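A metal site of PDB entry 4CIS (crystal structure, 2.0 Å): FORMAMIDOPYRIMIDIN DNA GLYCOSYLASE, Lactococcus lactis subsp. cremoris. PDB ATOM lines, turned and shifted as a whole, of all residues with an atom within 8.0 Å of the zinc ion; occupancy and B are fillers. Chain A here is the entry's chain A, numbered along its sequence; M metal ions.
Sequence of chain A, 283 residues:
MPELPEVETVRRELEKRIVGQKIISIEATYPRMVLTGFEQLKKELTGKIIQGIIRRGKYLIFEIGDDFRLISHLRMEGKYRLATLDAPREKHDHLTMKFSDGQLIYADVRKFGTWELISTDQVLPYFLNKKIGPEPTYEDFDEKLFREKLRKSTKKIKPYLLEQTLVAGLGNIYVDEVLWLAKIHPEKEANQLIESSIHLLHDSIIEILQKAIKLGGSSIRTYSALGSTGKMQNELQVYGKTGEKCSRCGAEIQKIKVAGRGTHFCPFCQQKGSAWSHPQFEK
The side-chain sulfur of Cys 269 sits close to the guanidinium group of Arg 248 (3.5 Å). The backbone NH (N) of Arg 248 lies close to the side-chain sulfur (SG) of Cys 246 (3.4 Å). N of Cys 246 sits at hydrogen-bond distance from O of Ala 251 (2.6 Å). The side-chain sulfur (SG) of Cys 246 lies close to the indole nitrogen (NE1) of Trp 180 (3.5 Å). SG of Cys 249 sits close to N of Ala 251 (3.4 Å). The backbone NH of Phe 268 lies close to the side-chain sulfur of Cys 266 (3.4 Å). OE1 of Gln 270 sits at hydrogen-bond distance from N of Cys 266 (2.8 Å).
Of the 18 residues printed, 4 come within 4 Å of the zinc ion. The nearest printed residue that does not touch the zinc ion is Arg 248 (4.5 Å).
The side-chain sulfur (SG) of Cys 269 binds the zinc ion, at 2.2 Å. The zinc ion is bound by the side-chain sulfur (SG) of Cys 246, at 2.3 Å. The side-chain sulfur (SG) of Cys 249 binds the zinc ion (2.3 Å). The zinc ion is bound by SG of Cys 266, 2.3 Å away. The zinc ion has four donor atoms within binding distance.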
ATOM      1  N   TRP A 180       6.063 -21.950 -28.737  1.00  0.00           N
ATOM      2  CA  TRP A 180       5.285 -20.909 -28.138  1.00  0.00           C
ATOM      3  C   TRP A 180       6.132 -19.674 -27.824  1.00  0.00           C
ATOM      4  O   TRP A 180       5.795 -18.555 -28.214  1.00  0.00           O
ATOM      5  CB  TRP A 180       4.573 -21.407 -26.867  1.00  0.00           C
ATOM      6  CG  TRP A 180       3.748 -20.316 -26.203  1.00  0.00           C
ATOM      7  CD1 TRP A 180       2.443 -20.007 -26.490  1.00  0.00           C
ATOM      8  CD2 TRP A 180       4.159 -19.402 -25.192  1.00  0.00           C
ATOM      9  NE1 TRP A 180       2.015 -18.949 -25.696  1.00  0.00           N
ATOM     10  CE2 TRP A 180       3.048 -18.589 -24.878  1.00  0.00           C
ATOM     11  CE3 TRP A 180       5.361 -19.231 -24.472  1.00  0.00           C
ATOM     12  CZ2 TRP A 180       3.120 -17.587 -23.921  1.00  0.00           C
ATOM     13  CZ3 TRP A 180       5.441 -18.297 -23.568  1.00  0.00           C
ATOM     14  CH2 TRP A 180       4.318 -17.450 -23.274  1.00  0.00           C
ATOM     15  N   LYS A 183       6.917 -17.912 -30.914  1.00  0.00           N
ATOM     16  CA  LYS A 183       5.785 -17.547 -31.751  1.00  0.00           C
ATOM     17  C   LYS A 183       5.770 -18.225 -33.130  1.00  0.00           C
ATOM     18  O   LYS A 183       5.493 -17.624 -34.129  1.00  0.00           O
ATOM     19  CB  LYS A 183       5.688 -16.001 -31.868  1.00  0.00           C
ATOM     20  CG  LYS A 183       5.492 -15.368 -30.507  1.00  0.00           C
ATOM     21  CD  LYS A 183       5.539 -13.831 -30.557  1.00  0.00           C
ATOM     22  CE  LYS A 183       5.430 -13.263 -29.144  1.00  0.00           C
ATOM     23  NZ  LYS A 183       5.800 -11.788 -29.002  1.00  0.00           N
ATOM     24  N   VAL A 238       2.206 -23.848 -22.363  1.00  0.00           N
ATOM     25  CA  VAL A 238       1.176 -24.491 -23.242  1.00  0.00           C
ATOM     26  C   VAL A 238       0.895 -25.980 -22.958  1.00  0.00           C
ATOM     27  O   VAL A 238      -0.238 -26.452 -23.172  1.00  0.00           O
ATOM     28  CB  VAL A 238       1.457 -24.333 -24.781  1.00  0.00           C
ATOM     29  CG1 VAL A 238       1.414 -22.878 -25.191  1.00  0.00           C
ATOM     30  CG2 VAL A 238       2.792 -24.925 -25.235  1.00  0.00           C
ATOM     31  N   LYS A 245      -6.096 -19.759 -20.855  1.00  0.00           N
ATOM     32  CA  LYS A 245      -5.723 -18.537 -21.550  1.00  0.00           C
ATOM     33  C   LYS A 245      -4.228 -18.398 -21.751  1.00  0.00           C
ATOM     34  O   LYS A 245      -3.474 -18.527 -20.795  1.00  0.00           O
ATOM     35  CB  LYS A 245      -6.188 -17.345 -20.768  1.00  0.00           C
ATOM     36  CG  LYS A 245      -7.677 -17.088 -20.893  1.00  0.00           C
ATOM     37  CD  LYS A 245      -8.041 -15.860 -20.080  1.00  0.00           C
ATOM     38  CE  LYS A 245      -9.455 -15.464 -20.332  1.00  0.00           C
ATOM     39  NZ  LYS A 245     -10.114 -15.188 -19.022  1.00  0.00           N
ATOM     40  N   CYS A 246      -3.803 -18.056 -22.968  1.00  0.00           N
ATOM     41  CA  CYS A 246      -2.384 -17.760 -23.247  1.00  0.00           C
ATOM     42  C   CYS A 246      -1.973 -16.636 -22.355  1.00  0.00           C
ATOM     43  O   CYS A 246      -2.642 -15.626 -22.336  1.00  0.00           O
ATOM     44  CB  CYS A 246      -2.153 -17.352 -24.738  1.00  0.00           C
ATOM     45  SG  CYS A 246      -0.543 -16.669 -25.155  1.00  0.00           S
ATOM     46  N   SER A 247      -0.871 -16.784 -21.636  1.00  0.00           N
ATOM     47  CA  SER A 247      -0.454 -15.727 -20.677  1.00  0.00           C
ATOM     48  C   SER A 247      -0.072 -14.462 -21.370  1.00  0.00           C
ATOM     49  O   SER A 247      -0.015 -13.448 -20.742  1.00  0.00           O
ATOM     50  CB  SER A 247       0.745 -16.192 -19.849  1.00  0.00           C
ATOM     51  OG  SER A 247       1.861 -16.468 -20.683  1.00  0.00           O
ATOM     52  N   ARG A 248       0.193 -14.530 -22.661  1.00  0.00           N
ATOM     53  CA  ARG A 248       0.683 -13.408 -23.462  1.00  0.00           C
ATOM     54  C   ARG A 248      -0.478 -12.659 -24.078  1.00  0.00           C
ATOM     55  O   ARG A 248      -0.525 -11.438 -23.986  1.00  0.00           O
ATOM     56  CB  ARG A 248       1.685 -13.920 -24.522  1.00  0.00           C
ATOM     57  CG  ARG A 248       2.646 -12.887 -25.079  1.00  0.00           C
ATOM     58  CD  ARG A 248       3.902 -13.570 -25.609  1.00  0.00           C
ATOM     59  NE  ARG A 248       3.520 -14.714 -26.414  1.00  0.00           N
ATOM     60  CZ  ARG A 248       4.318 -15.677 -26.883  1.00  0.00           C
ATOM     61  NH1 ARG A 248       5.622 -15.621 -26.724  1.00  0.00           N
ATOM     62  NH2 ARG A 248       3.757 -16.658 -27.577  1.00  0.00           N
ATOM     63  N   CYS A 249      -1.472 -13.351 -24.626  1.00  0.00           N
ATOM     64  CA  CYS A 249      -2.568 -12.658 -25.378  1.00  0.00           C
ATOM     65  C   CYS A 249      -4.011 -12.884 -24.900  1.00  0.00           C
ATOM     66  O   CYS A 249      -4.926 -12.164 -25.310  1.00  0.00           O
ATOM     67  CB  CYS A 249      -2.500 -12.975 -26.869  1.00  0.00           C
ATOM     68  SG  CYS A 249      -2.986 -14.656 -27.308  1.00  0.00           S
ATOM     69  N   GLY A 250      -4.209 -13.848 -24.041  1.00  0.00           N
ATOM     70  CA  GLY A 250      -5.537 -14.201 -23.554  1.00  0.00           C
ATOM     71  C   GLY A 250      -6.250 -15.215 -24.439  1.00  0.00           C
ATOM     72  O   GLY A 250      -7.359 -15.591 -24.107  1.00  0.00           O
ATOM     73  N   ALA A 251      -5.674 -15.646 -25.559  1.00  0.00           N
ATOM     74  CA  ALA A 251      -6.341 -16.641 -26.464  1.00  0.00           C
ATOM     75  C   ALA A 251      -6.403 -18.002 -25.772  1.00  0.00           C
ATOM     76  O   ALA A 251      -5.623 -18.217 -24.852  1.00  0.00           O
ATOM     77  CB  ALA A 251      -5.589 -16.756 -27.755  1.00  0.00           C
ATOM     78  N   GLU A 252      -7.336 -18.882 -26.176  1.00  0.00           N
ATOM     79  CA  GLU A 252      -7.446 -20.232 -25.654  1.00  0.00           C
ATOM     80  C   GLU A 252      -6.425 -21.153 -26.335  1.00  0.00           C
ATOM     81  O   GLU A 252      -6.372 -21.294 -27.560  1.00  0.00           O
ATOM     82  CB  GLU A 252      -8.854 -20.780 -25.813  1.00  0.00           C
ATOM     83  CG  GLU A 252      -9.843 -20.065 -24.905  1.00  0.00           C
ATOM     84  CD  GLU A 252     -11.264 -20.453 -25.132  1.00  0.00           C
ATOM     85  OE1 GLU A 252     -11.499 -21.387 -25.907  1.00  0.00           O
ATOM     86  OE2 GLU A 252     -12.148 -19.832 -24.565  1.00  0.00           O
ATOM     87  N   ILE A 253      -5.626 -21.818 -25.512  1.00  0.00           N
ATOM     88  CA  ILE A 253      -4.641 -22.709 -25.983  1.00  0.00           C
ATOM     89  C   ILE A 253      -5.359 -23.883 -26.653  1.00  0.00           C
ATOM     90  O   ILE A 253      -6.325 -24.405 -26.106  1.00  0.00           O
ATOM     91  CB  ILE A 253      -3.765 -23.184 -24.790  1.00  0.00           C
ATOM     92  CG1 ILE A 253      -3.029 -21.998 -24.173  1.00  0.00           C
ATOM     93  CG2 ILE A 253      -2.801 -24.317 -25.220  1.00  0.00           C
ATOM     94  CD1 ILE A 253      -2.160 -21.239 -25.136  1.00  0.00           C
ATOM     95  N   PHE A 265      -0.641 -25.310 -28.562  1.00  0.00           N
ATOM     96  CA  PHE A 265      -0.217 -24.007 -29.078  1.00  0.00           C
ATOM     97  C   PHE A 265      -1.249 -22.881 -28.892  1.00  0.00           C
ATOM     98  O   PHE A 265      -2.470 -23.108 -28.696  1.00  0.00           O
ATOM     99  CB  PHE A 265       0.147 -24.087 -30.565  1.00  0.00           C
ATOM    100  CG  PHE A 265      -1.059 -24.238 -31.466  1.00  0.00           C
ATOM    101  CD1 PHE A 265      -1.762 -25.440 -31.522  1.00  0.00           C
ATOM    102  CD2 PHE A 265      -1.479 -23.186 -32.249  1.00  0.00           C
ATOM    103  CE1 PHE A 265      -2.866 -25.568 -32.336  1.00  0.00           C
ATOM    104  CE2 PHE A 265      -2.602 -23.267 -33.012  1.00  0.00           C
ATOM    105  CZ  PHE A 265      -3.284 -24.479 -33.092  1.00  0.00           C
ATOM    106  N   CYS A 266      -0.753 -21.646 -28.967  1.00  0.00           N
ATOM    107  CA  CYS A 266      -1.626 -20.443 -28.994  1.00  0.00           C
ATOM    108  C   CYS A 266      -1.982 -20.096 -30.426  1.00  0.00           C
ATOM    109  O   CYS A 266      -1.087 -19.801 -31.208  1.00  0.00           O
ATOM    110  CB  CYS A 266      -0.938 -19.217 -28.391  1.00  0.00           C
ATOM    111  SG  CYS A 266      -2.066 -17.844 -28.511  1.00  0.00           S
ATOM    112  N   PRO A 267      -3.309 -20.057 -30.738  1.00  0.00           N
ATOM    113  CA  PRO A 267      -3.800 -19.830 -32.120  1.00  0.00           C
ATOM    114  C   PRO A 267      -3.656 -18.426 -32.591  1.00  0.00           C
ATOM    115  O   PRO A 267      -3.784 -18.203 -33.814  1.00  0.00           O
ATOM    116  CB  PRO A 267      -5.295 -20.190 -32.060  1.00  0.00           C
ATOM    117  CG  PRO A 267      -5.665 -20.070 -30.617  1.00  0.00           C
ATOM    118  CD  PRO A 267      -4.407 -20.426 -29.820  1.00  0.00           C
ATOM    119  N   PHE A 268      -3.415 -17.503 -31.646  1.00  0.00           N
ATOM    120  CA  PHE A 268      -3.049 -16.129 -31.999  1.00  0.00           C
ATOM    121  C   PHE A 268      -1.530 -15.851 -32.081  1.00  0.00           C
ATOM    122  O   PHE A 268      -1.080 -15.274 -33.065  1.00  0.00           O
ATOM    123  CB  PHE A 268      -3.681 -15.145 -31.039  1.00  0.00           C
ATOM    124  CG  PHE A 268      -3.450 -13.695 -31.434  1.00  0.00           C
ATOM    125  CD1 PHE A 268      -4.239 -13.089 -32.410  1.00  0.00           C
ATOM    126  CD2 PHE A 268      -2.431 -12.947 -30.846  1.00  0.00           C
ATOM    127  CE1 PHE A 268      -4.034 -11.749 -32.738  1.00  0.00           C
ATOM    128  CE2 PHE A 268      -2.193 -11.637 -31.203  1.00  0.00           C
ATOM    129  CZ  PHE A 268      -3.004 -11.021 -32.125  1.00  0.00           C
ATOM    130  N   CYS A 269      -0.784 -16.219 -31.036  1.00  0.00           N
ATOM    131  CA  CYS A 269       0.659 -15.979 -30.985  1.00  0.00           C
ATOM    132  C   CYS A 269       1.398 -16.895 -31.991  1.00  0.00           C
ATOM    133  O   CYS A 269       2.459 -16.535 -32.470  1.00  0.00           O
ATOM    134  CB  CYS A 269       1.212 -16.201 -29.563  1.00  0.00           C
ATOM    135  SG  CYS A 269       0.584 -15.127 -28.218  1.00  0.00           S
ATOM    136  N   GLN A 270       0.818 -18.055 -32.324  1.00  0.00           N
ATOM    137  CA  GLN A 270       1.450 -18.956 -33.294  1.00  0.00           C
ATOM    138  C   GLN A 270       0.560 -19.252 -34.481  1.00  0.00           C
ATOM    139  O   GLN A 270      -0.364 -20.079 -34.365  1.00  0.00           O
ATOM    140  CB  GLN A 270       1.774 -20.290 -32.606  1.00  0.00           C
ATOM    141  CG  GLN A 270       2.689 -20.108 -31.401  1.00  0.00           C
ATOM    142  CD  GLN A 270       2.709 -21.345 -30.530  1.00  0.00           C
ATOM    143  OE1 GLN A 270       1.976 -21.430 -29.534  1.00  0.00           O
ATOM    144  NE2 GLN A 270       3.485 -22.312 -30.918  1.00  0.00           N
HETATM  145 ZN    ZN M   1      -1.125 -16.074 -27.293  1.00  0.00          ZN
